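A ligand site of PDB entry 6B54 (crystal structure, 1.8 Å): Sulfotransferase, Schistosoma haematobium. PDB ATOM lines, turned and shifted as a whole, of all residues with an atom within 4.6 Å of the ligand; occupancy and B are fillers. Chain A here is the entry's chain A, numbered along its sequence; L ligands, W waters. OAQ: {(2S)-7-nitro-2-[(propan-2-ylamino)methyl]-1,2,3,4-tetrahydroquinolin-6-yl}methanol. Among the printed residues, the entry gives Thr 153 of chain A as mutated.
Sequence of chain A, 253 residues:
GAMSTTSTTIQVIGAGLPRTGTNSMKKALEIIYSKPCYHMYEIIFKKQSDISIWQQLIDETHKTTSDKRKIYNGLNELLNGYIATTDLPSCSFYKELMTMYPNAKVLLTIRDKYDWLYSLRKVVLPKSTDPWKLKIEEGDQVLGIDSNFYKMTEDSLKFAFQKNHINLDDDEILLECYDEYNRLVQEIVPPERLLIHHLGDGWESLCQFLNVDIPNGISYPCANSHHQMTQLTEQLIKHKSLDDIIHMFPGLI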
ATOM      1  N   PRO A  18      15.265 -22.891  16.802  1.00  0.00           N
ATOM      2  CA  PRO A  18      16.246 -22.656  15.737  1.00  0.00           C
ATOM      3  C   PRO A  18      15.679 -21.755  14.662  1.00  0.00           C
ATOM      4  O   PRO A  18      14.453 -21.759  14.456  1.00  0.00           O
ATOM      5  CB  PRO A  18      16.520 -24.060  15.166  1.00  0.00           C
ATOM      6  CG  PRO A  18      15.344 -24.878  15.580  1.00  0.00           C
ATOM      7  CD  PRO A  18      14.937 -24.322  16.936  1.00  0.00           C
ATOM      8  N   HIS A  39      25.457 -23.468  21.445  1.00  0.00           N
ATOM      9  CA  HIS A  39      24.680 -23.272  20.206  1.00  0.00           C
ATOM     10  C   HIS A  39      24.876 -24.533  19.392  1.00  0.00           C
ATOM     11  O   HIS A  39      25.808 -25.296  19.646  1.00  0.00           O
ATOM     12  CB  HIS A  39      25.167 -22.031  19.414  1.00  0.00           C
ATOM     13  CG  HIS A  39      24.291 -21.666  18.237  1.00  0.00           C
ATOM     14  ND1 HIS A  39      24.525 -22.129  16.954  1.00  0.00           N
ATOM     15  CD2 HIS A  39      23.175 -20.894  18.164  1.00  0.00           C
ATOM     16  CE1 HIS A  39      23.593 -21.653  16.139  1.00  0.00           C
ATOM     17  NE2 HIS A  39      22.764 -20.908  16.848  1.00  0.00           N
ATOM     18  N   MET A  40      24.020 -24.773  18.392  1.00  0.00           N
ATOM     19  CA  MET A  40      24.238 -25.963  17.556  1.00  0.00           C
ATOM     20  C   MET A  40      25.592 -25.898  16.865  1.00  0.00           C
ATOM     21  O   MET A  40      26.214 -26.939  16.595  1.00  0.00           O
ATOM     22  CB  MET A  40      23.123 -26.125  16.514  1.00  0.00           C
ATOM     23  CG  MET A  40      23.248 -27.421  15.674  1.00  0.00           C
ATOM     24  SD  MET A  40      22.906 -28.929  16.619  1.00  0.00           S
ATOM     25  CE  MET A  40      21.126 -28.926  16.809  1.00  0.00           C
ATOM     26  N   TYR A  41      26.059 -24.701  16.549  1.00  0.00           N
ATOM     27  CA  TYR A  41      27.394 -24.564  15.945  1.00  0.00           C
ATOM     28  C   TYR A  41      28.491 -25.160  16.850  1.00  0.00           C
ATOM     29  O   TYR A  41      29.493 -25.650  16.341  1.00  0.00           O
ATOM     30  CB  TYR A  41      27.728 -23.105  15.669  1.00  0.00           C
ATOM     31  CG  TYR A  41      27.259 -22.548  14.334  1.00  0.00           C
ATOM     32  CD1 TYR A  41      25.948 -22.712  13.916  1.00  0.00           C
ATOM     33  CD2 TYR A  41      28.128 -21.806  13.528  1.00  0.00           C
ATOM     34  CE1 TYR A  41      25.517 -22.159  12.703  1.00  0.00           C
ATOM     35  CE2 TYR A  41      27.706 -21.269  12.324  1.00  0.00           C
ATOM     36  CZ  TYR A  41      26.391 -21.451  11.922  1.00  0.00           C
ATOM     37  OH  TYR A  41      25.986 -20.906  10.719  1.00  0.00           O
ATOM     38  N   ILE A  44      28.261 -28.985  15.994  1.00  0.00           N
ATOM     39  CA  ILE A  44      28.653 -29.353  14.638  1.00  0.00           C
ATOM     40  C   ILE A  44      30.112 -29.105  14.376  1.00  0.00           C
ATOM     41  O   ILE A  44      30.797 -29.960  13.795  1.00  0.00           O
ATOM     42  CB  ILE A  44      27.812 -28.599  13.572  1.00  0.00           C
ATOM     43  CG1 ILE A  44      26.342 -29.009  13.695  1.00  0.00           C
ATOM     44  CG2 ILE A  44      28.367 -28.859  12.160  1.00  0.00           C
ATOM     45  CD1 ILE A  44      25.413 -28.171  12.826  1.00  0.00           C
ATOM     46  N   PHE A  45      30.625 -27.963  14.812  1.00  0.00           N
ATOM     47  CA  PHE A  45      31.966 -27.569  14.397  1.00  0.00           C
ATOM     48  C   PHE A  45      33.031 -27.782  15.463  1.00  0.00           C
ATOM     49  O   PHE A  45      34.204 -27.610  15.191  1.00  0.00           O
ATOM     50  CB  PHE A  45      31.975 -26.107  13.947  1.00  0.00           C
ATOM     51  CG  PHE A  45      31.097 -25.846  12.733  1.00  0.00           C
ATOM     52  CD1 PHE A  45      31.533 -26.200  11.460  1.00  0.00           C
ATOM     53  CD2 PHE A  45      29.848 -25.237  12.867  1.00  0.00           C
ATOM     54  CE1 PHE A  45      30.727 -25.961  10.329  1.00  0.00           C
ATOM     55  CE2 PHE A  45      29.052 -25.000  11.772  1.00  0.00           C
ATOM     56  CZ  PHE A  45      29.490 -25.357  10.490  1.00  0.00           C
ATOM     57  N   ASP A  87      19.573 -22.113  21.004  1.00  0.00           N
ATOM     58  CA  ASP A  87      19.368 -22.994  19.849  1.00  0.00           C
ATOM     59  C   ASP A  87      18.933 -24.401  20.245  1.00  0.00           C
ATOM     60  O   ASP A  87      18.946 -24.786  21.427  1.00  0.00           O
ATOM     61  CB  ASP A  87      20.655 -23.047  19.010  1.00  0.00           C
ATOM     62  CG  ASP A  87      20.441 -23.464  17.560  1.00  0.00           C
ATOM     63  OD1 ASP A  87      19.281 -23.682  17.113  1.00  0.00           O
ATOM     64  OD2 ASP A  87      21.469 -23.531  16.857  1.00  0.00           O
ATOM     65  N   LEU A  88      18.503 -25.164  19.239  1.00  0.00           N
ATOM     66  CA  LEU A  88      18.412 -26.615  19.310  1.00  0.00           C
ATOM     67  C   LEU A  88      19.770 -27.189  19.644  1.00  0.00           C
ATOM     68  O   LEU A  88      20.777 -26.635  19.201  1.00  0.00           O
ATOM     69  CB  LEU A  88      17.976 -27.185  17.974  1.00  0.00           C
ATOM     70  CG  LEU A  88      16.584 -27.698  17.660  1.00  0.00           C
ATOM     71  CD1 LEU A  88      16.722 -28.780  16.562  1.00  0.00           C
ATOM     72  CD2 LEU A  88      15.835 -28.192  18.865  1.00  0.00           C
ATOM     73  N   VAL A 123      17.352 -25.152   6.118  1.00  0.00           N
ATOM     74  CA  VAL A 123      18.569 -25.450   6.882  1.00  0.00           C
ATOM     75  C   VAL A 123      18.413 -26.655   7.801  1.00  0.00           C
ATOM     76  O   VAL A 123      19.254 -27.540   7.802  1.00  0.00           O
ATOM     77  CB  VAL A 123      19.008 -24.232   7.700  1.00  0.00           C
ATOM     78  CG1 VAL A 123      20.256 -24.556   8.526  1.00  0.00           C
ATOM     79  CG2 VAL A 123      19.273 -23.023   6.785  1.00  0.00           C
ATOM     80  N   VAL A 124      17.308 -26.707   8.530  1.00  0.00           N
ATOM     81  CA  VAL A 124      17.193 -27.593   9.654  1.00  0.00           C
ATOM     82  C   VAL A 124      16.291 -28.777   9.344  1.00  0.00           C
ATOM     83  O   VAL A 124      16.578 -29.905   9.751  1.00  0.00           O
ATOM     84  CB  VAL A 124      16.663 -26.840  10.890  1.00  0.00           C
ATOM     85  CG1 VAL A 124      16.455 -27.789  12.049  1.00  0.00           C
ATOM     86  CG2 VAL A 124      17.645 -25.714  11.277  1.00  0.00           C
ATOM     87  N   GLY A 139      26.690 -32.234   1.845  1.00  0.00           N
ATOM     88  CA  GLY A 139      27.454 -31.200   2.510  1.00  0.00           C
ATOM     89  C   GLY A 139      27.849 -31.617   3.925  1.00  0.00           C
ATOM     90  O   GLY A 139      29.001 -31.490   4.317  1.00  0.00           O
ATOM     91  N   ASP A 140      26.888 -32.103   4.696  1.00  0.00           N
ATOM     92  CA  ASP A 140      27.178 -32.505   6.068  1.00  0.00           C
ATOM     93  C   ASP A 140      28.208 -33.644   6.118  1.00  0.00           C
ATOM     94  O   ASP A 140      28.930 -33.785   7.112  1.00  0.00           O
ATOM     95  CB  ASP A 140      25.914 -32.936   6.794  1.00  0.00           C
ATOM     96  CG  ASP A 140      25.026 -31.776   7.158  1.00  0.00           C
ATOM     97  OD1 ASP A 140      25.524 -30.619   7.186  1.00  0.00           O
ATOM     98  OD2 ASP A 140      23.846 -32.027   7.448  1.00  0.00           O
ATOM     99  N   LEU A 143      31.568 -32.555   6.682  1.00  0.00           N
ATOM    100  CA  LEU A 143      31.813 -32.076   8.038  1.00  0.00           C
ATOM    101  C   LEU A 143      31.951 -33.245   8.974  1.00  0.00           C
ATOM    102  O   LEU A 143      32.192 -33.072  10.162  1.00  0.00           O
ATOM    103  CB  LEU A 143      30.684 -31.167   8.505  1.00  0.00           C
ATOM    104  CG  LEU A 143      30.439 -29.871   7.723  1.00  0.00           C
ATOM    105  CD1 LEU A 143      29.205 -29.142   8.266  1.00  0.00           C
ATOM    106  CD2 LEU A 143      31.668 -28.971   7.754  1.00  0.00           C
ATOM    107  N   PHE A 149      22.861 -37.497  13.430  1.00  0.00           N
ATOM    108  CA  PHE A 149      22.660 -36.086  13.686  1.00  0.00           C
ATOM    109  C   PHE A 149      21.191 -35.704  13.432  1.00  0.00           C
ATOM    110  O   PHE A 149      20.562 -35.013  14.235  1.00  0.00           O
ATOM    111  CB  PHE A 149      23.589 -35.233  12.829  1.00  0.00           C
ATOM    112  CG  PHE A 149      23.374 -33.761  13.002  1.00  0.00           C
ATOM    113  CD1 PHE A 149      23.725 -33.134  14.195  1.00  0.00           C
ATOM    114  CD2 PHE A 149      22.791 -33.016  11.995  1.00  0.00           C
ATOM    115  CE1 PHE A 149      23.496 -31.769  14.362  1.00  0.00           C
ATOM    116  CE2 PHE A 149      22.562 -31.671  12.148  1.00  0.00           C
ATOM    117  CZ  PHE A 149      22.911 -31.039  13.327  1.00  0.00           C
ATOM    118  N   THR A 153      18.288 -34.059  15.991  1.00  0.00           N
ATOM    119  CA  THR A 153      17.639 -32.767  15.801  1.00  0.00           C
ATOM    120  C   THR A 153      16.115 -32.946  15.665  1.00  0.00           C
ATOM    121  O   THR A 153      15.340 -32.148  16.190  1.00  0.00           O
ATOM    122  CB  THR A 153      18.182 -31.989  14.576  1.00  0.00           C
ATOM    123  OG1 THR A 153      18.035 -32.781  13.401  1.00  0.00           O
ATOM    124  CG2 THR A 153      19.633 -31.649  14.762  1.00  0.00           C
ATOM    125  N   MET A 229      23.897 -20.317   4.599  1.00  0.00           N
ATOM    126  CA  MET A 229      23.914 -21.753   4.792  1.00  0.00           C
ATOM    127  C   MET A 229      23.822 -22.497   3.446  1.00  0.00           C
ATOM    128  O   MET A 229      24.423 -23.552   3.264  1.00  0.00           O
ATOM    129  CB  MET A 229      22.789 -22.177   5.739  1.00  0.00           C
ATOM    130  CG  MET A 229      23.024 -21.780   7.202  1.00  0.00           C
ATOM    131  SD  MET A 229      24.577 -22.472   7.842  1.00  0.00           S
ATOM    132  CE  MET A 229      25.672 -21.086   7.615  1.00  0.00           C
ATOM    133  N   LEU A 232      27.211 -22.297   1.869  1.00  0.00           N
ATOM    134  CA  LEU A 232      28.149 -23.157   2.593  1.00  0.00           C
ATOM    135  C   LEU A 232      27.959 -24.612   2.154  1.00  0.00           C
ATOM    136  O   LEU A 232      28.927 -25.350   1.998  1.00  0.00           O
ATOM    137  CB  LEU A 232      27.993 -23.017   4.122  1.00  0.00           C
ATOM    138  CG  LEU A 232      28.802 -23.957   5.021  1.00  0.00           C
ATOM    139  CD1 LEU A 232      30.298 -23.625   4.935  1.00  0.00           C
ATOM    140  CD2 LEU A 232      28.294 -23.884   6.452  1.00  0.00           C
ATOM    141  N   THR A 233      26.706 -25.015   1.977  1.00  0.00           N
ATOM    142  CA  THR A 233      26.391 -26.352   1.525  1.00  0.00           C
ATOM    143  C   THR A 233      26.992 -26.569   0.108  1.00  0.00           C
ATOM    144  O   THR A 233      27.642 -27.577  -0.146  1.00  0.00           O
ATOM    145  CB  THR A 233      24.840 -26.602   1.487  1.00  0.00           C
ATOM    146  OG1 THR A 233      24.280 -26.406   2.779  1.00  0.00           O
ATOM    147  CG2 THR A 233      24.534 -28.025   1.049  1.00  0.00           C
ATOM    148  N   LEU A 236      30.840 -26.684   0.254  1.00  0.00           N
ATOM    149  CA  LEU A 236      31.342 -27.912   0.866  1.00  0.00           C
ATOM    150  C   LEU A 236      31.281 -29.035  -0.156  1.00  0.00           C
ATOM    151  O   LEU A 236      32.161 -29.899  -0.219  1.00  0.00           O
ATOM    152  CB  LEU A 236      30.546 -28.296   2.115  1.00  0.00           C
ATOM    153  CG  LEU A 236      30.821 -27.510   3.425  1.00  0.00           C
ATOM    154  CD1 LEU A 236      29.729 -27.779   4.408  1.00  0.00           C
ATOM    155  CD2 LEU A 236      32.185 -27.885   4.047  1.00  0.00           C
HETATM  156  C1  OAQ L   1      21.927 -25.281  12.624  1.00  0.00           C
HETATM  157  C2  OAQ L   1      20.911 -26.116  13.120  1.00  0.00           C
HETATM  158  C3  OAQ L   1      20.708 -27.361  12.485  1.00  0.00           C
HETATM  159  C4  OAQ L   1      21.488 -27.735  11.407  1.00  0.00           C
HETATM  160  C5  OAQ L   1      22.481 -26.902  10.928  1.00  0.00           C
HETATM  161  C6  OAQ L   1      22.720 -25.657  11.529  1.00  0.00           C
HETATM  162  C7  OAQ L   1      24.213 -26.471   9.186  1.00  0.00           C
HETATM  163  C8  OAQ L   1      24.859 -25.569  10.269  1.00  0.00           C
HETATM  164  C9  OAQ L   1      23.741 -24.790  11.044  1.00  0.00           C
HETATM  165  C10 OAQ L   1      20.155 -25.656  14.202  1.00  0.00           C
HETATM  166  C11 OAQ L   1      25.252 -27.295   8.419  1.00  0.00           C
HETATM  167  C12 OAQ L   1      26.578 -28.113   5.911  1.00  0.00           C
HETATM  168  C13 OAQ L   1      25.047 -26.177   5.783  1.00  0.00           C
HETATM  169  C14 OAQ L   1      25.121 -27.692   6.032  1.00  0.00           C
HETATM  170  N1  OAQ L   1      23.235 -27.357   9.833  1.00  0.00           N
HETATM  171  N2  OAQ L   1      19.797 -28.256  12.865  1.00  0.00           N
HETATM  172  N3  OAQ L   1      24.581 -28.081   7.349  1.00  0.00           N
HETATM  173  O1  OAQ L   1      19.640 -29.278  12.054  1.00  0.00           O
HETATM  174  O2  OAQ L   1      19.014 -28.188  14.083  1.00  0.00           O
HETATM  175  O3  OAQ L   1      20.620 -24.361  14.555  1.00  0.00           O
HETATM  176  O   HOH W   1      20.804 -22.235  12.895  1.00  0.00           O
HETATM  177  O   HOH W   2      18.787 -31.426  10.909  1.00  0.00           O
HETATM  178  O   HOH W   3      21.882 -27.155   6.729  1.00  0.00           O
HETATM  179  O   HOH W   4      22.597 -29.956   8.655  1.00  0.00           O
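The side-chain carboxylate (OD2) of Asp 87 lies within hydrogen-bond range of an oxygen (O3) of the ligand.
The side-chain carboxylate (OD1) of Asp 140 is in salt-bridge range of a nitrogen (N3) of the ligand (2.7 Å).
NE2 of His 39 lies close to OD2 of Asp 87 (2.9 Å).
The backbone carbonyl oxygen (O) of Phe 149 is in hydrogen-bond range of the side-chain hydroxyl (OG1) of Thr 153.
The backbone NH (N) of Met 40 lies close to the side-chain carboxylate (OD2) of Asp 87 (3.2 Å).
OH of Tyr 41 sits close to SD of Met 229.
The backbone NH of Tyr 41 sits at hydrogen-bond distance from a ring nitrogen (ND1) of His 39, at 3.0 Å.
O of Met 229 is in hydrogen-bond range of OG1 of Thr 233 (2.9 Å).
Residues that only touch the ligand: Thr 233 (3.1 Å), Val 124 (3.3 Å), Leu 88 (3.4 Å), Leu 236 (3.5 Å), Met 40 (3.5 Å), Thr 153 (3.6 Å), Tyr 41 (3.6 Å), Leu 143 (3.7 Å), Ile 44 (3.7 Å), Met 229 (3.7 Å) and Phe 149 (3.8 Å).
Hydrophobic or aromatic side chains that line the ligand: Met 40, Tyr 41, Ile 44, Leu 88, Val 124, Leu 143, Phe 149, Met 229 and Leu 236.
Water W2 lies within hydrogen-bond range of O1 of the ligand (2.6 Å), O of Val 124 (2.9 Å) and OG1 of Thr 153 (2.9 Å).
Water W3 bridges the backbone carbonyl oxygen (O) of Val 123 (2.9 Å) and a nitrogen (N3) of the ligand (2.9 Å).
Water W4 lies within hydrogen-bond range of OD2 of Asp 140 (2.7 Å) and N1 of the ligand (2.9 Å).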
